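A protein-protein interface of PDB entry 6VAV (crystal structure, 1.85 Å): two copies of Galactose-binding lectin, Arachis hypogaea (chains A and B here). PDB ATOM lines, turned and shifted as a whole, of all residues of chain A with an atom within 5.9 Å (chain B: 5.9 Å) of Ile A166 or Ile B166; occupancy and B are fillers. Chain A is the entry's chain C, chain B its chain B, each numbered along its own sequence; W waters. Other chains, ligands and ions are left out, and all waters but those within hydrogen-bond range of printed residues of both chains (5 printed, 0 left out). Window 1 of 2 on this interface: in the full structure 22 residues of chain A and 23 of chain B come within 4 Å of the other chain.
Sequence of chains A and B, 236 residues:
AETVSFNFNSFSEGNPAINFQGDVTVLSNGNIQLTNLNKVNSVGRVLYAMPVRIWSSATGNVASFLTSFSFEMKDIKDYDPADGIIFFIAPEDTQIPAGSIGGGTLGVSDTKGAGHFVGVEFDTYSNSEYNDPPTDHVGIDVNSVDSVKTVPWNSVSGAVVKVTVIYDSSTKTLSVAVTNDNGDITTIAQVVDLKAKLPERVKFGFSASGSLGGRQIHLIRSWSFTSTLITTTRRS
Of the 14 printed residues of chain B, 9 touch a printed residue of chain A.
Among the printed residues, 14 pairs touch across the chains.
Among the printed residues, no Asp or Glu carboxylate lies within 4 Å of a Lys or Arg side-chain nitrogen of the other chain.
OG1 of Thr A187 lies within hydrogen-bond range of OD1 of Asp B168 (2.7 Å).
The side-chain hydroxyl (OG1) of Thr B187 is in hydrogen-bond range of the side-chain carboxylate (OD1) of Asp A168 (2.7 Å).
Water W5 lies within hydrogen-bond range of the side-chain hydroxyl of Ser A175 (2.5 Å), the backbone carbonyl oxygen of Thr B173 (2.7 Å), the side-chain hydroxyl of Ser B175 (2.9 Å) and the backbone carbonyl oxygen of Ile B166 (3.0 Å).
Water W3 lies within hydrogen-bond range of the side-chain carboxylate (OD1) of Asp B168 (2.7 Å) and the side-chain hydroxyl (OG1) of Thr A187 (3.5 Å).
Water W4 lies within hydrogen-bond range of OD1 of Asp A168 (2.7 Å) and OG1 of Thr B187 (3.3 Å).
Water W1 lies within hydrogen-bond range of OG of Ser B175 (2.8 Å), O of Thr A173 (2.9 Å) and O of Ile A166 (3.1 Å).
Water W2 bridges O of Thr A187 (2.8 Å) and OD1 of Asp B168 (3.4 Å).
Ile B166 touches Thr A164 (CD1 to O, 3.7 Å).
Ile A166 touches Thr B164 (CD1 to O, 3.8 Å).
Ile B166 touches Ile A166 (CD1 to CD1, 3.9 Å).
Ser B175 touches Ile A166 (O to CD1, 3.9 Å).
Thr B173 touches Thr A173.
OG of Ser A175 touches CG2 of Ile B166, at 3.5 Å.
Ser B175 touches Ser A175.
CB of Ala A177 touches CD2 of Leu B66 (3.9 Å).
Ala A177 touches Ile B166 (CB to CD1, 3.8 Å).
Thr A187 touches Tyr B167.
Thr A164 touches Ile B166, and with the chains exchanged Ile A166 touches Thr B164.
Ile A166 touches its own counterpart, Ile B166.
Ile A166 touches Ala B177, and with the chains exchanged Ala A177 touches Ile B166.
Ser A175 touches its own counterpart, Ser B175.
Positions printed for both chains: 65, 66, 67, 164, 165, 166, 167, 168, 173, 174, 175, 176, 177 and 187.
The backbone carbonyl oxygen (O) of Phe B65 sits at hydrogen-bond distance from the backbone NH (N) of Tyr B167.
N of Ala B177 sits at hydrogen-bond distance from O of Thr B164, at 2.9 Å.
The backbone carbonyl oxygen (O) of Ile B166 is in hydrogen-bond range of the backbone NH (N) of Ser B175 (2.8 Å).
The backbone carbonyl oxygen of Thr A164 lies within hydrogen-bond range of the backbone NH of Ala A177 (2.9 Å).
The backbone NH (N) of Ser A175 is in hydrogen-bond range of the backbone carbonyl oxygen (O) of Ile A166 (2.8 Å).
O of Thr A173 sits at hydrogen-bond distance from N of Asp A168 (2.9 Å).
Ile A166 touches just these residues of chain B: Thr B164, Ile B166, Ser B175 and Ala B177.
Of the printed residues of chain A, Ile B166 touches Thr A164, Ile A166, Ser A175 and Ala A177.
Of the printed residues of chain A, Thr B164 touches Thr A164 (3.8 Å) and Ile A166 (3.8 Å).
Of the printed residues of chain A, Thr B187 touches Asp A168 (2.7 Å).
Of the printed residues of chain A, Ala B177 touches Ile A166.
Leu A174 touches none of the printed residues of chain B.
The nearest residue of chain B that does not touch Ile A166 is Thr B187 (4.2 Å).
The nearest residue of chain A that does not touch Ile B166 is Thr A187 (4.1 Å).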
ATOM      1  N   PHE A  65       9.042 -10.826   3.522  1.00  0.00           N
ATOM      2  CA  PHE A  65       9.334  -9.503   4.050  1.00  0.00           C
ATOM      3  C   PHE A  65      10.276  -9.572   5.226  1.00  0.00           C
ATOM      4  O   PHE A  65      10.384 -10.597   5.891  1.00  0.00           O
ATOM      5  CB  PHE A  65       8.046  -8.689   4.395  1.00  0.00           C
ATOM      6  CG  PHE A  65       7.134  -9.158   5.508  1.00  0.00           C
ATOM      7  CD1 PHE A  65       7.479  -8.961   6.841  1.00  0.00           C
ATOM      8  CD2 PHE A  65       5.874  -9.683   5.224  1.00  0.00           C
ATOM      9  CE1 PHE A  65       6.617  -9.357   7.876  1.00  0.00           C
ATOM     10  CE2 PHE A  65       5.008 -10.057   6.260  1.00  0.00           C
ATOM     11  CZ  PHE A  65       5.398  -9.915   7.577  1.00  0.00           C
ATOM     12  N   LEU A  66      11.012  -8.478   5.421  1.00  0.00           N
ATOM     13  CA  LEU A  66      11.904  -8.210   6.551  1.00  0.00           C
ATOM     14  C   LEU A  66      11.509  -6.860   7.124  1.00  0.00           C
ATOM     15  O   LEU A  66      11.470  -5.868   6.391  1.00  0.00           O
ATOM     16  CB  LEU A  66      13.395  -8.228   6.145  1.00  0.00           C
ATOM     17  CG  LEU A  66      14.396  -7.712   7.211  1.00  0.00           C
ATOM     18  CD1 LEU A  66      14.448  -8.635   8.445  1.00  0.00           C
ATOM     19  CD2 LEU A  66      15.796  -7.493   6.631  1.00  0.00           C
ATOM     20  N   THR A  67      11.207  -6.820   8.418  1.00  0.00           N
ATOM     21  CA  THR A  67      10.814  -5.583   9.060  1.00  0.00           C
ATOM     22  C   THR A  67      11.415  -5.501  10.454  1.00  0.00           C
ATOM     23  O   THR A  67      11.523  -6.501  11.160  1.00  0.00           O
ATOM     24  CB  THR A  67       9.275  -5.372   9.048  1.00  0.00           C
ATOM     25  OG1 THR A  67       8.993  -4.032   9.447  1.00  0.00           O
ATOM     26  CG2 THR A  67       8.491  -6.361   9.946  1.00  0.00           C
ATOM     27  N   THR A 164      12.768  -7.677  15.299  1.00  0.00           N
ATOM     28  CA  THR A 164      13.048  -8.040  13.935  1.00  0.00           C
ATOM     29  C   THR A 164      12.050  -9.136  13.558  1.00  0.00           C
ATOM     30  O   THR A 164      11.881 -10.109  14.289  1.00  0.00           O
ATOM     31  CB  THR A 164      14.523  -8.448  13.719  1.00  0.00           C
ATOM     32  OG1 THR A 164      15.351  -7.304  13.944  1.00  0.00           O
ATOM     33  CG2 THR A 164      14.776  -8.930  12.318  1.00  0.00           C
ATOM     34  N   VAL A 165      11.415  -8.983  12.410  1.00  0.00           N
ATOM     35  CA  VAL A 165      10.437  -9.944  11.909  1.00  0.00           C
ATOM     36  C   VAL A 165      10.814 -10.364  10.479  1.00  0.00           C
ATOM     37  O   VAL A 165      11.084  -9.519   9.619  1.00  0.00           O
ATOM     38  CB  VAL A 165       8.971  -9.424  11.979  1.00  0.00           C
ATOM     39  CG1 VAL A 165       7.987 -10.494  11.512  1.00  0.00           C
ATOM     40  CG2 VAL A 165       8.596  -8.924  13.388  1.00  0.00           C
ATOM     41  N   ILE A 166      10.819 -11.679  10.233  1.00  0.00           N
ATOM     42  CA  ILE A 166      11.061 -12.274   8.923  1.00  0.00           C
ATOM     43  C   ILE A 166       9.845 -13.101   8.544  1.00  0.00           C
ATOM     44  O   ILE A 166       9.464 -14.009   9.273  1.00  0.00           O
ATOM     45  CB  ILE A 166      12.368 -13.131   8.844  1.00  0.00           C
ATOM     46  CG1 ILE A 166      13.643 -12.289   9.178  1.00  0.00           C
ATOM     47  CG2 ILE A 166      12.494 -13.858   7.487  1.00  0.00           C
ATOM     48  CD1 ILE A 166      14.984 -13.141   9.402  1.00  0.00           C
ATOM     49  N   TYR A 167       9.262 -12.806   7.402  1.00  0.00           N
ATOM     50  CA  TYR A 167       8.239 -13.671   6.838  1.00  0.00           C
ATOM     51  C   TYR A 167       8.826 -14.327   5.589  1.00  0.00           C
ATOM     52  O   TYR A 167       9.175 -13.637   4.629  1.00  0.00           O
ATOM     53  CB  TYR A 167       6.925 -12.956   6.543  1.00  0.00           C
ATOM     54  CG  TYR A 167       5.864 -13.917   6.055  1.00  0.00           C
ATOM     55  CD1 TYR A 167       5.237 -14.799   6.937  1.00  0.00           C
ATOM     56  CD2 TYR A 167       5.556 -14.016   4.700  1.00  0.00           C
ATOM     57  CE1 TYR A 167       4.308 -15.735   6.484  1.00  0.00           C
ATOM     58  CE2 TYR A 167       4.621 -14.945   4.236  1.00  0.00           C
ATOM     59  CZ  TYR A 167       3.989 -15.795   5.134  1.00  0.00           C
ATOM     60  OH  TYR A 167       3.048 -16.694   4.670  1.00  0.00           O
ATOM     61  N   ASP A 168       8.979 -15.655   5.628  1.00  0.00           N
ATOM     62  CA  ASP A 168       9.503 -16.423   4.517  1.00  0.00           C
ATOM     63  C   ASP A 168       8.331 -17.037   3.747  1.00  0.00           C
ATOM     64  O   ASP A 168       7.663 -17.944   4.257  1.00  0.00           O
ATOM     65  CB  ASP A 168      10.493 -17.493   5.003  1.00  0.00           C
ATOM     66  CG  ASP A 168      10.964 -18.380   3.860  1.00  0.00           C
ATOM     67  OD1 ASP A 168      11.689 -17.874   2.973  1.00  0.00           O
ATOM     68  OD2 ASP A 168      10.546 -19.552   3.811  1.00  0.00           O
ATOM     69  N   THR A 173       6.507 -19.119   7.083  1.00  0.00           N
ATOM     70  CA  THR A 173       6.948 -18.919   8.455  1.00  0.00           C
ATOM     71  C   THR A 173       7.120 -17.451   8.785  1.00  0.00           C
ATOM     72  O   THR A 173       7.853 -16.731   8.102  1.00  0.00           O
ATOM     73  CB  THR A 173       8.257 -19.662   8.750  1.00  0.00           C
ATOM     74  OG1 THR A 173       8.092 -21.056   8.480  1.00  0.00           O
ATOM     75  CG2 THR A 173       8.725 -19.487  10.198  1.00  0.00           C
ATOM     76  N   LEU A 174       6.461 -17.041   9.868  1.00  0.00           N
ATOM     77  CA  LEU A 174       6.585 -15.715  10.477  1.00  0.00           C
ATOM     78  C   LEU A 174       7.514 -15.890  11.668  1.00  0.00           C
ATOM     79  O   LEU A 174       7.133 -16.564  12.624  1.00  0.00           O
ATOM     80  CB  LEU A 174       5.204 -15.153  10.894  1.00  0.00           C
ATOM     81  CG  LEU A 174       5.190 -13.709  11.410  1.00  0.00           C
ATOM     82  CD1 LEU A 174       5.442 -12.719  10.272  1.00  0.00           C
ATOM     83  CD2 LEU A 174       3.871 -13.395  12.089  1.00  0.00           C
ATOM     84  N   SER A 175       8.749 -15.381  11.584  1.00  0.00           N
ATOM     85  CA  SER A 175       9.723 -15.499  12.670  1.00  0.00           C
ATOM     86  C   SER A 175       9.990 -14.127  13.318  1.00  0.00           C
ATOM     87  O   SER A 175      10.143 -13.127  12.596  1.00  0.00           O
ATOM     88  CB  SER A 175      11.006 -16.106  12.144  1.00  0.00           C
ATOM     89  OG  SER A 175      11.526 -16.850  13.218  1.00  0.00           O
ATOM     90  N   VAL A 176       9.984 -14.072  14.661  1.00  0.00           N
ATOM     91  CA  VAL A 176      10.119 -12.840  15.459  1.00  0.00           C
ATOM     92  C   VAL A 176      11.283 -12.946  16.450  1.00  0.00           C
ATOM     93  O   VAL A 176      11.346 -13.926  17.207  1.00  0.00           O
ATOM     94  CB  VAL A 176       8.788 -12.545  16.225  1.00  0.00           C
ATOM     95  CG1 VAL A 176       8.842 -11.206  16.950  1.00  0.00           C
ATOM     96  CG2 VAL A 176       7.571 -12.585  15.299  1.00  0.00           C
ATOM     97  N   ALA A 177      12.150 -11.913  16.502  1.00  0.00           N
ATOM     98  CA  ALA A 177      13.245 -11.821  17.472  1.00  0.00           C
ATOM     99  C   ALA A 177      13.097 -10.495  18.210  1.00  0.00           C
ATOM    100  O   ALA A 177      12.947  -9.439  17.579  1.00  0.00           O
ATOM    101  CB  ALA A 177      14.601 -11.942  16.794  1.00  0.00           C
ATOM    102  N   THR A 187      12.526 -15.280  21.115  1.00  0.00           N
ATOM    103  CA  THR A 187      12.057 -15.550  19.756  1.00  0.00           C
ATOM    104  C   THR A 187      10.746 -16.303  19.777  1.00  0.00           C
ATOM    105  O   THR A 187      10.451 -17.038  20.718  1.00  0.00           O
ATOM    106  CB  THR A 187      13.073 -16.319  18.886  1.00  0.00           C
ATOM    107  OG1 THR A 187      13.196 -17.658  19.367  1.00  0.00           O
ATOM    108  CG2 THR A 187      14.442 -15.606  18.743  1.00  0.00           C
ATOM    109  N   PHE B  65      18.607 -17.636  18.795  1.00  0.00           N
ATOM    110  CA  PHE B  65      19.606 -16.632  18.499  1.00  0.00           C
ATOM    111  C   PHE B  65      19.132 -15.680  17.392  1.00  0.00           C
ATOM    112  O   PHE B  65      18.250 -16.004  16.587  1.00  0.00           O
ATOM    113  CB  PHE B  65      20.993 -17.223  18.176  1.00  0.00           C
ATOM    114  CG  PHE B  65      21.179 -18.057  16.925  1.00  0.00           C
ATOM    115  CD1 PHE B  65      21.292 -17.452  15.678  1.00  0.00           C
ATOM    116  CD2 PHE B  65      21.369 -19.430  17.012  1.00  0.00           C
ATOM    117  CE1 PHE B  65      21.509 -18.212  14.534  1.00  0.00           C
ATOM    118  CE2 PHE B  65      21.594 -20.194  15.877  1.00  0.00           C
ATOM    119  CZ  PHE B  65      21.655 -19.586  14.634  1.00  0.00           C
ATOM    120  N   LEU B  66      19.691 -14.477  17.429  1.00  0.00           N
ATOM    121  CA  LEU B  66      19.526 -13.421  16.446  1.00  0.00           C
ATOM    122  C   LEU B  66      20.918 -12.948  16.061  1.00  0.00           C
ATOM    123  O   LEU B  66      21.716 -12.576  16.927  1.00  0.00           O
ATOM    124  CB  LEU B  66      18.653 -12.253  16.950  1.00  0.00           C
ATOM    125  CG  LEU B  66      18.626 -10.969  16.086  1.00  0.00           C
ATOM    126  CD1 LEU B  66      17.968 -11.197  14.722  1.00  0.00           C
ATOM    127  CD2 LEU B  66      17.879  -9.845  16.790  1.00  0.00           C
ATOM    128  N   THR B  67      21.213 -12.950  14.767  1.00  0.00           N
ATOM    129  CA  THR B  67      22.526 -12.511  14.305  1.00  0.00           C
ATOM    130  C   THR B  67      22.389 -11.742  13.001  1.00  0.00           C
ATOM    131  O   THR B  67      21.542 -12.051  12.168  1.00  0.00           O
ATOM    132  CB  THR B  67      23.537 -13.691  14.223  1.00  0.00           C
ATOM    133  OG1 THR B  67      24.849 -13.170  14.018  1.00  0.00           O
ATOM    134  CG2 THR B  67      23.193 -14.730  13.157  1.00  0.00           C
ATOM    135  N   THR B 164      20.345 -11.032   7.972  1.00  0.00           N
ATOM    136  CA  THR B 164      19.754 -11.200   9.271  1.00  0.00           C
ATOM    137  C   THR B 164      19.326 -12.657   9.381  1.00  0.00           C
ATOM    138  O   THR B 164      18.703 -13.191   8.475  1.00  0.00           O
ATOM    139  CB  THR B 164      18.600 -10.202   9.520  1.00  0.00           C
ATOM    140  OG1 THR B 164      19.147  -8.876   9.532  1.00  0.00           O
ATOM    141  CG2 THR B 164      17.913 -10.453  10.868  1.00  0.00           C
ATOM    142  N   VAL B 165      19.701 -13.304  10.484  1.00  0.00           N
ATOM    143  CA  VAL B 165      19.355 -14.704  10.748  1.00  0.00           C
ATOM    144  C   VAL B 165      18.675 -14.816  12.123  1.00  0.00           C
ATOM    145  O   VAL B 165      19.168 -14.287  13.124  1.00  0.00           O
ATOM    146  CB  VAL B 165      20.584 -15.658  10.656  1.00  0.00           C
ATOM    147  CG1 VAL B 165      20.166 -17.112  10.882  1.00  0.00           C
ATOM    148  CG2 VAL B 165      21.350 -15.486   9.331  1.00  0.00           C
ATOM    149  N   ILE B 166      17.553 -15.558  12.154  1.00  0.00           N
ATOM    150  CA  ILE B 166      16.805 -15.860  13.367  1.00  0.00           C
ATOM    151  C   ILE B 166      16.713 -17.374  13.510  1.00  0.00           C
ATOM    152  O   ILE B 166      16.202 -18.053  12.625  1.00  0.00           O
ATOM    153  CB  ILE B 166      15.371 -15.209  13.413  1.00  0.00           C
ATOM    154  CG1 ILE B 166      15.432 -13.665  13.362  1.00  0.00           C
ATOM    155  CG2 ILE B 166      14.556 -15.699  14.640  1.00  0.00           C
ATOM    156  CD1 ILE B 166      14.090 -12.915  13.153  1.00  0.00           C
ATOM    157  N   TYR B 167      17.152 -17.883  14.647  1.00  0.00           N
ATOM    158  CA  TYR B 167      16.909 -19.264  14.979  1.00  0.00           C
ATOM    159  C   TYR B 167      15.944 -19.303  16.163  1.00  0.00           C
ATOM    160  O   TYR B 167      16.261 -18.797  17.251  1.00  0.00           O
ATOM    161  CB  TYR B 167      18.187 -20.048  15.273  1.00  0.00           C
ATOM    162  CG  TYR B 167      17.907 -21.514  15.519  1.00  0.00           C
ATOM    163  CD1 TYR B 167      17.571 -22.357  14.463  1.00  0.00           C
ATOM    164  CD2 TYR B 167      17.870 -22.034  16.811  1.00  0.00           C
ATOM    165  CE1 TYR B 167      17.254 -23.700  14.689  1.00  0.00           C
ATOM    166  CE2 TYR B 167      17.558 -23.374  17.049  1.00  0.00           C
ATOM    167  CZ  TYR B 167      17.254 -24.203  15.982  1.00  0.00           C
ATOM    168  OH  TYR B 167      16.950 -25.519  16.214  1.00  0.00           O
ATOM    169  N   ASP B 168      14.756 -19.861  15.923  1.00  0.00           N
ATOM    170  CA  ASP B 168      13.717 -19.993  16.936  1.00  0.00           C
ATOM    171  C   ASP B 168      13.774 -21.415  17.498  1.00  0.00           C
ATOM    172  O   ASP B 168      13.418 -22.374  16.808  1.00  0.00           O
ATOM    173  CB  ASP B 168      12.321 -19.662  16.354  1.00  0.00           C
ATOM    174  CG  ASP B 168      11.221 -19.892  17.370  1.00  0.00           C
ATOM    175  OD1 ASP B 168      11.185 -19.155  18.379  1.00  0.00           O
ATOM    176  OD2 ASP B 168      10.442 -20.854  17.193  1.00  0.00           O
ATOM    177  N   THR B 173      13.291 -23.497  13.740  1.00  0.00           N
ATOM    178  CA  THR B 173      13.355 -22.801  12.455  1.00  0.00           C
ATOM    179  C   THR B 173      14.524 -21.856  12.368  1.00  0.00           C
ATOM    180  O   THR B 173      14.675 -20.948  13.198  1.00  0.00           O
ATOM    181  CB  THR B 173      12.062 -22.031  12.145  1.00  0.00           C
ATOM    182  OG1 THR B 173      10.967 -22.944  12.195  1.00  0.00           O
ATOM    183  CG2 THR B 173      12.112 -21.355  10.774  1.00  0.00           C
ATOM    184  N   LEU B 174      15.335 -22.053  11.306  1.00  0.00           N
ATOM    185  CA  LEU B 174      16.424 -21.170  10.928  1.00  0.00           C
ATOM    186  C   LEU B 174      15.887 -20.295   9.790  1.00  0.00           C
ATOM    187  O   LEU B 174      15.609 -20.821   8.714  1.00  0.00           O
ATOM    188  CB  LEU B 174      17.669 -21.979  10.495  1.00  0.00           C
ATOM    189  CG  LEU B 174      18.931 -21.172  10.231  1.00  0.00           C
ATOM    190  CD1 LEU B 174      19.521 -20.605  11.537  1.00  0.00           C
ATOM    191  CD2 LEU B 174      19.980 -22.035   9.499  1.00  0.00           C
ATOM    192  N   SER B 175      15.680 -18.987  10.043  1.00  0.00           N
ATOM    193  CA  SER B 175      15.160 -18.044   9.038  1.00  0.00           C
ATOM    194  C   SER B 175      16.229 -17.028   8.654  1.00  0.00           C
ATOM    195  O   SER B 175      16.905 -16.486   9.526  1.00  0.00           O
ATOM    196  CB  SER B 175      13.907 -17.330   9.548  1.00  0.00           C
ATOM    197  OG  SER B 175      12.888 -18.264   9.833  1.00  0.00           O
ATOM    198  N   VAL B 176      16.368 -16.764   7.345  1.00  0.00           N
ATOM    199  CA  VAL B 176      17.416 -15.897   6.783  1.00  0.00           C
ATOM    200  C   VAL B 176      16.806 -14.830   5.873  1.00  0.00           C
ATOM    201  O   VAL B 176      16.071 -15.168   4.957  1.00  0.00           O
ATOM    202  CB  VAL B 176      18.464 -16.761   5.962  1.00  0.00           C
ATOM    203  CG1 VAL B 176      19.631 -15.910   5.448  1.00  0.00           C
ATOM    204  CG2 VAL B 176      18.993 -17.941   6.776  1.00  0.00           C
ATOM    205  N   ALA B 177      17.196 -13.576   6.063  1.00  0.00           N
ATOM    206  CA  ALA B 177      16.797 -12.468   5.197  1.00  0.00           C
ATOM    207  C   ALA B 177      18.070 -11.804   4.658  1.00  0.00           C
ATOM    208  O   ALA B 177      18.978 -11.456   5.426  1.00  0.00           O
ATOM    209  CB  ALA B 177      15.909 -11.470   5.947  1.00  0.00           C
ATOM    210  N   THR B 187      14.657 -14.325   0.956  1.00  0.00           N
ATOM    211  CA  THR B 187      14.557 -15.058   2.223  1.00  0.00           C
ATOM    212  C   THR B 187      14.658 -16.558   1.973  1.00  0.00           C
ATOM    213  O   THR B 187      14.262 -17.051   0.923  1.00  0.00           O
ATOM    214  CB  THR B 187      13.254 -14.758   3.024  1.00  0.00           C
ATOM    215  OG1 THR B 187      12.123 -15.265   2.311  1.00  0.00           O
ATOM    216  CG2 THR B 187      13.088 -13.295   3.414  1.00  0.00           C
HETATM  217  O   HOH W   1      10.713 -16.802   8.756  1.00  0.00           O
HETATM  218  O   HOH W   2       8.945 -19.430  20.950  1.00  0.00           O
HETATM  219  O   HOH W   3      11.529 -20.373  20.752  1.00  0.00           O
HETATM  220  O   HOH W   4      10.647 -17.617   0.480  1.00  0.00           O
HETATM  221  O   HOH W   5      13.229 -18.672  12.704  1.00  0.00           O
